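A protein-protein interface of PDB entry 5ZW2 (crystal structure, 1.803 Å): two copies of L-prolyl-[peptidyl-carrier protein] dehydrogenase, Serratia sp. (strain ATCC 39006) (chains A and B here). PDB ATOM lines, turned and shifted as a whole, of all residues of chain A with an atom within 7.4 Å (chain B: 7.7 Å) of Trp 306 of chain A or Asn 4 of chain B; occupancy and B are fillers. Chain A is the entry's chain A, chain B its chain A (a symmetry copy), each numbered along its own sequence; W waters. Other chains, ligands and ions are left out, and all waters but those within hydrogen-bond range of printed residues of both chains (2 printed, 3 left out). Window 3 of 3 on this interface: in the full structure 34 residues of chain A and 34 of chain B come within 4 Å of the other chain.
OD2 of Asp 2 of chain B lies within hydrogen-bond range of N of Asn 4 of chain B (2.8 Å).
Met 1 of chain A touches Asp 2 of chain B, and with the chains exchanged Asp 2 of chain A touches Met 1 of chain B.
Met 1 of chain A touches Tyr 302 of chain B, and with the chains exchanged Tyr 302 of chain A touches Met 1 of chain B.
Asp 2 of chain B touches its own counterpart, Asp 2 of chain A.
Of the 13 pairs that touch across the chains among the printed residues, 5 have their exchanged pair printed and touching as well.
Hydrophobic or aromatic side chains of chain A that line the printed part of chain B: Met 1, Tyr 302 and Trp 306.
Of the 11 printed residues of chain B, 5 touch a printed residue of chain A.
Along chain B the printed residues that touch a printed residue of chain A span positions 1 to 302.
Among the printed residues, pairs that only touch across the chains: Met 1 of chain A with Asp 2 of chain B, Met 1 of chain A with Phe 3 of chain B, Met 1 of chain A with Tyr 302 of chain B, Asp 2 of chain A with Met 1 of chain B, Tyr 302 of chain A with Met 1 of chain B, Tyr 302 of chain A with Phe 3 of chain B, Arg 303 of chain A with Phe 3 of chain B, Trp 306 of chain A with Asp 2 of chain B, Trp 306 of chain A with Phe 3 of chain B and Trp 306 of chain A with Asn 4 of chain B.
Of chain B, only Met 1 (3.5 Å), Asp 2 (3.6 Å), Phe 3 (3.5 Å) and Asn 4 (3.5 Å) come within 4 Å of Trp 306 of chain A.
Asn 4 of chain B touches just these residues of chain A: Met 1 (2.7 Å) and Trp 306 (3.5 Å).
Of the printed residues of chain B, Arg 303 of chain A touches Phe 3 (3.6 Å).
Of the printed residues of chain A, Phe 3 of chain B touches Met 1 (3.2 Å), Tyr 302 (3.8 Å), Arg 303 (3.6 Å) and Trp 306 (3.5 Å).
Of the printed residues of chain A, Met 1 of chain B touches Asp 2, Tyr 302 and Trp 306.
Printed residues of chain B within 4 Å of Met 1 of chain A: Asp 2 (3.3 Å), Phe 3 (3.2 Å), Asn 4 (2.7 Å) and Tyr 302 (3.7 Å).
Leu 67 of chain B touches none of the printed residues of chain A.
The nearest residue of chain B that does not touch Trp 306 of chain A is Leu 5 of chain B (7.0 Å).
The nearest residue of chain A that does not touch Asn 4 of chain B is Gln 312 of chain A (4.4 Å).
The backbone NH (N) of Met 1 of chain A sits at hydrogen-bond distance from the backbone carbonyl oxygen (O) of Asn 4 of chain B, at 2.7 Å.
The backbone NH (N) of Asp 2 of chain A is in hydrogen-bond range of the backbone carbonyl oxygen (O) of Asp 2 of chain B, 2.9 Å away.
The backbone carbonyl oxygen (O) of Met 1 of chain B is in hydrogen-bond range of the indole nitrogen (NE1) of Trp 306 of chain A.
Water W1 lies within hydrogen-bond range of the side-chain carboxylate (OD1) of Asp 2 of chain B (2.8 Å), the indole nitrogen (NE1) of Trp 306 of chain A (2.9 Å) and the backbone carbonyl oxygen (O) of Met 1 of chain B (3.3 Å).
Water W2 lies within hydrogen-bond range of O of Phe 3 of chain B and NH1 of Arg 303 of chain A.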
ATOM      1  N   MET A   1       5.418   0.191 -15.867  1.00  0.00           N
ATOM      2  CA  MET A   1       5.082   0.988 -14.672  1.00  0.00           C
ATOM      3  C   MET A   1       4.872   2.464 -15.040  1.00  0.00           C
ATOM      4  O   MET A   1       5.682   3.035 -15.773  1.00  0.00           O
ATOM      5  CB  MET A   1       6.212   0.841 -13.666  1.00  0.00           C
ATOM      6  CG  MET A   1       5.962   1.543 -12.406  1.00  0.00           C
ATOM      7  SD  MET A   1       6.560   0.475 -11.133  1.00  0.00           S
ATOM      8  CE  MET A   1       5.227  -0.601 -11.292  1.00  0.00           C
ATOM      9  N   ASP A   2       3.785   3.072 -14.542  1.00  0.00           N
ATOM     10  CA  ASP A   2       3.433   4.441 -14.890  1.00  0.00           C
ATOM     11  C   ASP A   2       2.576   4.974 -13.752  1.00  0.00           C
ATOM     12  O   ASP A   2       1.658   4.276 -13.302  1.00  0.00           O
ATOM     13  CB  ASP A   2       2.643   4.503 -16.197  1.00  0.00           C
ATOM     14  CG  ASP A   2       2.355   5.943 -16.622  1.00  0.00           C
ATOM     15  OD1 ASP A   2       3.005   6.451 -17.536  1.00  0.00           O
ATOM     16  OD2 ASP A   2       1.481   6.576 -16.036  1.00  0.00           O
ATOM     17  N   GLN A   9      -9.050   9.674 -17.014  1.00  0.00           N
ATOM     18  CA  GLN A   9      -9.118   9.679 -15.541  1.00  0.00           C
ATOM     19  C   GLN A   9      -8.948  11.070 -14.962  1.00  0.00           C
ATOM     20  O   GLN A   9      -9.647  11.421 -13.999  1.00  0.00           O
ATOM     21  CB  GLN A   9      -8.061   8.724 -14.991  1.00  0.00           C
ATOM     22  CG  GLN A   9      -8.535   7.311 -15.176  1.00  0.00           C
ATOM     23  CD  GLN A   9      -7.470   6.267 -14.859  1.00  0.00           C
ATOM     24  OE1 GLN A   9      -6.259   6.497 -15.024  1.00  0.00           O
ATOM     25  NE2 GLN A   9      -7.951   5.075 -14.466  1.00  0.00           N
ATOM     26  N   ALA A  66     -12.733   0.076 -11.376  1.00  0.00           N
ATOM     27  CA  ALA A  66     -12.581   0.377  -9.949  1.00  0.00           C
ATOM     28  C   ALA A  66     -11.696   1.589  -9.746  1.00  0.00           C
ATOM     29  O   ALA A  66     -11.981   2.438  -8.875  1.00  0.00           O
ATOM     30  CB  ALA A  66     -12.022  -0.841  -9.196  1.00  0.00           C
ATOM     31  N   LEU A  67     -10.600   1.692 -10.508  1.00  0.00           N
ATOM     32  CA  LEU A  67      -9.741   2.859 -10.339  1.00  0.00           C
ATOM     33  C   LEU A  67     -10.483   4.133 -10.713  1.00  0.00           C
ATOM     34  O   LEU A  67     -10.444   5.125  -9.975  1.00  0.00           O
ATOM     35  CB  LEU A  67      -8.442   2.725 -11.148  1.00  0.00           C
ATOM     36  CG  LEU A  67      -7.447   3.869 -11.061  1.00  0.00           C
ATOM     37  CD1 LEU A  67      -7.118   4.161  -9.536  1.00  0.00           C
ATOM     38  CD2 LEU A  67      -6.123   3.490 -11.831  1.00  0.00           C
ATOM     39  N   ASP A  68     -11.207   4.123 -11.845  1.00  0.00           N
ATOM     40  CA  ASP A  68     -12.018   5.296 -12.190  1.00  0.00           C
ATOM     41  C   ASP A  68     -12.991   5.657 -11.079  1.00  0.00           C
ATOM     42  O   ASP A  68     -13.214   6.838 -10.802  1.00  0.00           O
ATOM     43  CB  ASP A  68     -12.892   5.041 -13.422  1.00  0.00           C
ATOM     44  CG  ASP A  68     -12.125   4.736 -14.697  1.00  0.00           C
ATOM     45  OD1 ASP A  68     -11.027   5.271 -14.900  1.00  0.00           O
ATOM     46  OD2 ASP A  68     -12.720   3.981 -15.539  1.00  0.00           O
ATOM     47  N   MET A 300      -1.294   2.645  -2.476  1.00  0.00           N
ATOM     48  CA  MET A 300      -1.835   1.308  -2.194  1.00  0.00           C
ATOM     49  C   MET A 300      -3.265   1.183  -2.702  1.00  0.00           C
ATOM     50  O   MET A 300      -3.678   0.116  -3.202  1.00  0.00           O
ATOM     51  CB  MET A 300      -1.764   1.039  -0.674  1.00  0.00           C
ATOM     52  CG  MET A 300      -0.332   0.954  -0.148  1.00  0.00           C
ATOM     53  SD  MET A 300       0.445  -0.624  -0.661  1.00  0.00           S
ATOM     54  CE  MET A 300      -0.436  -1.800   0.444  1.00  0.00           C
ATOM     55  N   LEU A 301      -4.050   2.247  -2.539  1.00  0.00           N
ATOM     56  CA  LEU A 301      -5.449   2.194  -3.019  1.00  0.00           C
ATOM     57  C   LEU A 301      -5.479   2.057  -4.536  1.00  0.00           C
ATOM     58  O   LEU A 301      -6.213   1.225  -5.097  1.00  0.00           O
ATOM     59  CB  LEU A 301      -6.197   3.466  -2.601  1.00  0.00           C
ATOM     60  CG  LEU A 301      -7.591   3.621  -3.244  1.00  0.00           C
ATOM     61  CD1 LEU A 301      -8.518   2.522  -2.762  1.00  0.00           C
ATOM     62  CD2 LEU A 301      -8.177   4.946  -2.985  1.00  0.00           C
ATOM     63  N   TYR A 302      -4.704   2.894  -5.212  1.00  0.00           N
ATOM     64  CA  TYR A 302      -4.710   2.864  -6.671  1.00  0.00           C
ATOM     65  C   TYR A 302      -4.268   1.512  -7.168  1.00  0.00           C
ATOM     66  O   TYR A 302      -4.803   1.011  -8.157  1.00  0.00           O
ATOM     67  CB  TYR A 302      -3.773   3.906  -7.262  1.00  0.00           C
ATOM     68  CG  TYR A 302      -4.236   5.356  -7.102  1.00  0.00           C
ATOM     69  CD1 TYR A 302      -5.486   5.647  -6.569  1.00  0.00           C
ATOM     70  CD2 TYR A 302      -3.383   6.388  -7.413  1.00  0.00           C
ATOM     71  CE1 TYR A 302      -5.896   7.001  -6.357  1.00  0.00           C
ATOM     72  CE2 TYR A 302      -3.783   7.738  -7.256  1.00  0.00           C
ATOM     73  CZ  TYR A 302      -5.054   8.014  -6.746  1.00  0.00           C
ATOM     74  OH  TYR A 302      -5.431   9.329  -6.577  1.00  0.00           O
ATOM     75  N   ARG A 303      -3.274   0.918  -6.518  1.00  0.00           N
ATOM     76  CA  ARG A 303      -2.822  -0.388  -7.008  1.00  0.00           C
ATOM     77  C   ARG A 303      -3.874  -1.460  -6.769  1.00  0.00           C
ATOM     78  O   ARG A 303      -4.074  -2.343  -7.623  1.00  0.00           O
ATOM     79  CB  ARG A 303      -1.477  -0.791  -6.378  1.00  0.00           C
ATOM     80  CG  ARG A 303      -1.077  -2.201  -6.874  1.00  0.00           C
ATOM     81  CD  ARG A 303       0.397  -2.451  -6.571  1.00  0.00           C
ATOM     82  NE  ARG A 303       0.466  -2.901  -5.206  1.00  0.00           N
ATOM     83  CZ  ARG A 303       1.565  -3.330  -4.579  1.00  0.00           C
ATOM     84  NH1 ARG A 303       2.744  -3.367  -5.196  1.00  0.00           N
ATOM     85  NH2 ARG A 303       1.471  -3.725  -3.321  1.00  0.00           N
ATOM     86  N   ALA A 304      -4.530  -1.440  -5.598  1.00  0.00           N
ATOM     87  CA  ALA A 304      -5.592  -2.394  -5.349  1.00  0.00           C
ATOM     88  C   ALA A 304      -6.653  -2.293  -6.428  1.00  0.00           C
ATOM     89  O   ALA A 304      -7.121  -3.321  -6.940  1.00  0.00           O
ATOM     90  CB  ALA A 304      -6.239  -2.177  -3.960  1.00  0.00           C
ATOM     91  N   CYS A 305      -7.064  -1.053  -6.781  1.00  0.00           N
ATOM     92  CA  CYS A 305      -8.145  -0.927  -7.761  1.00  0.00           C
ATOM     93  C   CYS A 305      -7.665  -1.352  -9.136  1.00  0.00           C
ATOM     94  O   CYS A 305      -8.411  -1.985  -9.898  1.00  0.00           O
ATOM     95  CB  CYS A 305      -8.646   0.510  -7.853  1.00  0.00           C
ATOM     96  SG  CYS A 305      -9.449   1.054  -6.293  1.00  0.00           S
ATOM     97  N   TRP A 306      -6.451  -0.954  -9.479  1.00  0.00           N
ATOM     98  CA  TRP A 306      -5.855  -1.358 -10.748  1.00  0.00           C
ATOM     99  C   TRP A 306      -5.772  -2.883 -10.863  1.00  0.00           C
ATOM    100  O   TRP A 306      -6.163  -3.458 -11.885  1.00  0.00           O
ATOM    101  CB  TRP A 306      -4.473  -0.706 -10.882  1.00  0.00           C
ATOM    102  CG  TRP A 306      -3.728  -1.077 -12.164  1.00  0.00           C
ATOM    103  CD1 TRP A 306      -3.788  -0.456 -13.379  1.00  0.00           C
ATOM    104  CD2 TRP A 306      -2.813  -2.141 -12.285  1.00  0.00           C
ATOM    105  NE1 TRP A 306      -2.907  -1.099 -14.283  1.00  0.00           N
ATOM    106  CE2 TRP A 306      -2.319  -2.138 -13.611  1.00  0.00           C
ATOM    107  CE3 TRP A 306      -2.343  -3.100 -11.381  1.00  0.00           C
ATOM    108  CZ2 TRP A 306      -1.392  -3.054 -14.048  1.00  0.00           C
ATOM    109  CZ3 TRP A 306      -1.414  -4.017 -11.833  1.00  0.00           C
ATOM    110  CH2 TRP A 306      -0.959  -3.983 -13.165  1.00  0.00           C
ATOM    111  N   LYS A 307      -5.304  -3.562  -9.811  1.00  0.00           N
ATOM    112  CA  LYS A 307      -5.294  -5.031  -9.823  1.00  0.00           C
ATOM    113  C   LYS A 307      -6.680  -5.605 -10.096  1.00  0.00           C
ATOM    114  O   LYS A 307      -6.836  -6.537 -10.898  1.00  0.00           O
ATOM    115  CB  LYS A 307      -4.762  -5.563  -8.490  1.00  0.00           C
ATOM    116  CG  LYS A 307      -3.288  -5.487  -8.362  1.00  0.00           C
ATOM    117  CD  LYS A 307      -2.840  -6.048  -6.993  1.00  0.00           C
ATOM    118  CE  LYS A 307      -1.348  -6.349  -6.950  1.00  0.00           C
ATOM    119  NZ  LYS A 307      -0.946  -7.202  -5.763  1.00  0.00           N
ATOM    120  N   HIS A 308      -7.707  -5.093  -9.416  1.00  0.00           N
ATOM    121  CA  HIS A 308      -9.062  -5.545  -9.719  1.00  0.00           C
ATOM    122  C   HIS A 308      -9.384  -5.332 -11.196  1.00  0.00           C
ATOM    123  O   HIS A 308      -9.906  -6.233 -11.868  1.00  0.00           O
ATOM    124  CB  HIS A 308     -10.104  -4.811  -8.851  1.00  0.00           C
ATOM    125  CG  HIS A 308     -11.492  -5.066  -9.308  1.00  0.00           C
ATOM    126  ND1 HIS A 308     -12.275  -6.051  -8.765  1.00  0.00           N
ATOM    127  CD2 HIS A 308     -12.215  -4.516 -10.315  1.00  0.00           C
ATOM    128  CE1 HIS A 308     -13.444  -6.073  -9.385  1.00  0.00           C
ATOM    129  NE2 HIS A 308     -13.436  -5.150 -10.329  1.00  0.00           N
ATOM    130  N   ASP A 309      -9.078  -4.143 -11.725  1.00  0.00           N
ATOM    131  CA  ASP A 309      -9.375  -3.854 -13.135  1.00  0.00           C
ATOM    132  C   ASP A 309      -8.635  -4.805 -14.074  1.00  0.00           C
ATOM    133  O   ASP A 309      -9.119  -5.069 -15.192  1.00  0.00           O
ATOM    134  CB  ASP A 309      -9.051  -2.402 -13.485  1.00  0.00           C
ATOM    135  CG  ASP A 309     -10.067  -1.434 -12.832  1.00  0.00           C
ATOM    136  OD1 ASP A 309     -11.147  -1.944 -12.442  1.00  0.00           O
ATOM    137  OD2 ASP A 309      -9.763  -0.240 -12.654  1.00  0.00           O
ATOM    138  N   GLN A 310      -7.460  -5.285 -13.672  1.00  0.00           N
ATOM    139  CA  GLN A 310      -6.684  -6.224 -14.478  1.00  0.00           C
ATOM    140  C   GLN A 310      -7.195  -7.649 -14.375  1.00  0.00           C
ATOM    141  O   GLN A 310      -6.638  -8.543 -15.037  1.00  0.00           O
ATOM    142  CB  GLN A 310      -5.210  -6.180 -14.074  1.00  0.00           C
ATOM    143  CG  GLN A 310      -4.557  -4.832 -14.338  1.00  0.00           C
ATOM    144  CD  GLN A 310      -4.296  -4.652 -15.811  1.00  0.00           C
ATOM    145  OE1 GLN A 310      -4.764  -3.699 -16.432  1.00  0.00           O
ATOM    146  NE2 GLN A 310      -3.572  -5.607 -16.402  1.00  0.00           N
ATOM    147  N   GLY A 311      -8.210  -7.890 -13.559  1.00  0.00           N
ATOM    148  CA  GLY A 311      -8.680  -9.235 -13.290  1.00  0.00           C
ATOM    149  C   GLY A 311      -7.802 -10.040 -12.366  1.00  0.00           C
ATOM    150  O   GLY A 311      -7.896 -11.272 -12.350  1.00  0.00           O
ATOM    151  N   GLN A 312      -6.921  -9.398 -11.618  1.00  0.00           N
ATOM    152  CA  GLN A 312      -6.065 -10.115 -10.684  1.00  0.00           C
ATOM    153  C   GLN A 312      -6.756 -10.254  -9.325  1.00  0.00           C
ATOM    154  O   GLN A 312      -7.758  -9.595  -9.033  1.00  0.00           O
ATOM    155  CB  GLN A 312      -4.722  -9.413 -10.532  1.00  0.00           C
ATOM    156  CG  GLN A 312      -3.901  -9.287 -11.801  1.00  0.00           C
ATOM    157  CD  GLN A 312      -2.594  -8.598 -11.530  1.00  0.00           C
ATOM    158  OE1 GLN A 312      -2.124  -8.545 -10.375  1.00  0.00           O
ATOM    159  NE2 GLN A 312      -1.975  -8.071 -12.572  1.00  0.00           N
ATOM    160  N   ALA A 314      -7.298  -9.245  -5.872  1.00  0.00           N
ATOM    161  CA  ALA A 314      -6.941  -8.016  -5.178  1.00  0.00           C
ATOM    162  C   ALA A 314      -7.382  -8.055  -3.730  1.00  0.00           C
ATOM    163  O   ALA A 314      -7.324  -7.011  -3.061  1.00  0.00           O
ATOM    164  CB  ALA A 314      -7.550  -6.795  -5.893  1.00  0.00           C
ATOM    165  N   MET B   1      -1.947   4.983 -15.581  1.00  0.00           N
ATOM    166  CA  MET B   1      -1.444   4.299 -14.373  1.00  0.00           C
ATOM    167  C   MET B   1      -1.277   2.794 -14.627  1.00  0.00           C
ATOM    168  O   MET B   1      -2.177   2.162 -15.183  1.00  0.00           O
ATOM    169  CB  MET B   1      -2.424   4.548 -13.239  1.00  0.00           C
ATOM    170  CG  MET B   1      -1.997   3.966 -11.965  1.00  0.00           C
ATOM    171  SD  MET B   1      -2.421   5.153 -10.728  1.00  0.00           S
ATOM    172  CE  MET B   1      -1.129   6.200 -11.170  1.00  0.00           C
ATOM    173  N   ASP B   2      -0.127   2.229 -14.229  1.00  0.00           N
ATOM    174  CA  ASP B   2       0.182   0.831 -14.492  1.00  0.00           C
ATOM    175  C   ASP B   2       1.192   0.401 -13.439  1.00  0.00           C
ATOM    176  O   ASP B   2       2.159   1.132 -13.188  1.00  0.00           O
ATOM    177  CB  ASP B   2       0.784   0.641 -15.885  1.00  0.00           C
ATOM    178  CG  ASP B   2       1.020  -0.835 -16.207  1.00  0.00           C
ATOM    179  OD1 ASP B   2       0.252  -1.423 -16.971  1.00  0.00           O
ATOM    180  OD2 ASP B   2       1.970  -1.416 -15.691  1.00  0.00           O
ATOM    181  N   PHE B   3       0.929  -0.736 -12.789  1.00  0.00           N
ATOM    182  CA  PHE B   3       1.805  -1.247 -11.734  1.00  0.00           C
ATOM    183  C   PHE B   3       2.604  -2.491 -12.133  1.00  0.00           C
ATOM    184  O   PHE B   3       3.203  -3.133 -11.269  1.00  0.00           O
ATOM    185  CB  PHE B   3       0.989  -1.500 -10.477  1.00  0.00           C
ATOM    186  CG  PHE B   3       0.435  -0.225  -9.906  1.00  0.00           C
ATOM    187  CD1 PHE B   3       1.214   0.567  -9.046  1.00  0.00           C
ATOM    188  CD2 PHE B   3      -0.850   0.202 -10.236  1.00  0.00           C
ATOM    189  CE1 PHE B   3       0.704   1.782  -8.515  1.00  0.00           C
ATOM    190  CE2 PHE B   3      -1.337   1.402  -9.738  1.00  0.00           C
ATOM    191  CZ  PHE B   3      -0.577   2.190  -8.874  1.00  0.00           C
ATOM    192  N   ASN B   4       2.700  -2.794 -13.421  1.00  0.00           N
ATOM    193  CA  ASN B   4       3.557  -3.873 -13.892  1.00  0.00           C
ATOM    194  C   ASN B   4       4.945  -3.346 -14.254  1.00  0.00           C
ATOM    195  O   ASN B   4       5.103  -2.236 -14.757  1.00  0.00           O
ATOM    196  CB  ASN B   4       2.957  -4.536 -15.143  1.00  0.00           C
ATOM    197  CG  ASN B   4       1.809  -5.520 -14.821  1.00  0.00           C
ATOM    198  OD1 ASN B   4       1.820  -6.214 -13.789  1.00  0.00           O
ATOM    199  ND2 ASN B   4       0.803  -5.551 -15.704  1.00  0.00           N
ATOM    200  N   LEU B   5       5.959  -4.192 -14.054  1.00  0.00           N
ATOM    201  CA  LEU B   5       7.237  -3.935 -14.707  1.00  0.00           C
ATOM    202  C   LEU B   5       7.102  -4.191 -16.205  1.00  0.00           C
ATOM    203  O   LEU B   5       6.335  -5.053 -16.626  1.00  0.00           O
ATOM    204  CB  LEU B   5       8.320  -4.859 -14.155  1.00  0.00           C
ATOM    205  CG  LEU B   5       8.631  -4.797 -12.645  1.00  0.00           C
ATOM    206  CD1 LEU B   5       9.876  -5.641 -12.394  1.00  0.00           C
ATOM    207  CD2 LEU B   5       8.852  -3.382 -12.333  1.00  0.00           C
ATOM    208  N   SER B   6       7.893  -3.482 -16.997  1.00  0.00           N
ATOM    209  CA  SER B   6       8.048  -3.845 -18.396  1.00  0.00           C
ATOM    210  C   SER B   6       8.731  -5.208 -18.508  1.00  0.00           C
ATOM    211  O   SER B   6       9.328  -5.721 -17.549  1.00  0.00           O
ATOM    212  CB  SER B   6       8.847  -2.767 -19.143  1.00  0.00           C
ATOM    213  OG  SER B   6      10.222  -2.741 -18.745  1.00  0.00           O
ATOM    214  N   ASN B   7       8.654  -5.804 -19.699  1.00  0.00           N
ATOM    215  CA  ASN B   7       9.382  -7.061 -19.896  1.00  0.00           C
ATOM    216  C   ASN B   7      10.886  -6.859 -19.722  1.00  0.00           C
ATOM    217  O   ASN B   7      11.571  -7.697 -19.117  1.00  0.00           O
ATOM    218  CB  ASN B   7       9.085  -7.649 -21.280  1.00  0.00           C
ATOM    219  CG  ASN B   7       7.675  -8.214 -21.398  1.00  0.00           C
ATOM    220  OD1 ASN B   7       7.027  -8.556 -20.398  1.00  0.00           O
ATOM    221  ND2 ASN B   7       7.194  -8.316 -22.629  1.00  0.00           N
ATOM    222  N   GLN B   9      12.284  -4.661 -17.823  1.00  0.00           N
ATOM    223  CA  GLN B   9      12.556  -4.528 -16.380  1.00  0.00           C
ATOM    224  C   GLN B   9      12.476  -5.857 -15.655  1.00  0.00           C
ATOM    225  O   GLN B   9      13.305  -6.120 -14.769  1.00  0.00           O
ATOM    226  CB  GLN B   9      11.579  -3.519 -15.781  1.00  0.00           C
ATOM    227  CG  GLN B   9      12.014  -2.132 -16.162  1.00  0.00           C
ATOM    228  CD  GLN B   9      10.996  -1.056 -15.800  1.00  0.00           C
ATOM    229  OE1 GLN B   9       9.775  -1.292 -15.774  1.00  0.00           O
ATOM    230  NE2 GLN B   9      11.519   0.164 -15.591  1.00  0.00           N
ATOM    231  N   SER B  10      11.484  -6.702 -15.990  1.00  0.00           N
ATOM    232  CA  SER B  10      11.451  -8.035 -15.401  1.00  0.00           C
ATOM    233  C   SER B  10      12.742  -8.800 -15.679  1.00  0.00           C
ATOM    234  O   SER B  10      13.241  -9.513 -14.802  1.00  0.00           O
ATOM    235  CB  SER B  10      10.240  -8.808 -15.903  1.00  0.00           C
ATOM    236  OG  SER B  10       9.060  -8.205 -15.396  1.00  0.00           O
ATOM    237  N   LEU B  67      14.668   3.887 -12.375  1.00  0.00           N
ATOM    238  CA  LEU B  67      13.848   2.747 -11.980  1.00  0.00           C
ATOM    239  C   LEU B  67      14.540   1.439 -12.331  1.00  0.00           C
ATOM    240  O   LEU B  67      14.610   0.521 -11.505  1.00  0.00           O
ATOM    241  CB  LEU B  67      12.449   2.813 -12.610  1.00  0.00           C
ATOM    242  CG  LEU B  67      11.483   1.689 -12.278  1.00  0.00           C
ATOM    243  CD1 LEU B  67      11.371   1.544 -10.702  1.00  0.00           C
ATOM    244  CD2 LEU B  67      10.063   2.003 -12.889  1.00  0.00           C
ATOM    245  N   TYR B 302       9.571   3.228  -6.224  1.00  0.00           N
ATOM    246  CA  TYR B 302       9.374   3.120  -7.666  1.00  0.00           C
ATOM    247  C   TYR B 302       8.859   4.423  -8.221  1.00  0.00           C
ATOM    248  O   TYR B 302       9.248   4.825  -9.318  1.00  0.00           O
ATOM    249  CB  TYR B 302       8.371   2.034  -8.020  1.00  0.00           C
ATOM    250  CG  TYR B 302       8.862   0.602  -7.791  1.00  0.00           C
ATOM    251  CD1 TYR B 302      10.176   0.354  -7.411  1.00  0.00           C
ATOM    252  CD2 TYR B 302       7.980  -0.449  -7.882  1.00  0.00           C
ATOM    253  CE1 TYR B 302      10.619  -0.976  -7.131  1.00  0.00           C
ATOM    254  CE2 TYR B 302       8.407  -1.780  -7.655  1.00  0.00           C
ATOM    255  CZ  TYR B 302       9.739  -2.016  -7.302  1.00  0.00           C
ATOM    256  OH  TYR B 302      10.144  -3.311  -7.065  1.00  0.00           O
HETATM  257  O   HOH W   1      -2.420  -0.519 -17.056  1.00  0.00           O
HETATM  258  O   HOH W   2       3.774  -2.690  -8.180  1.00  0.00           O
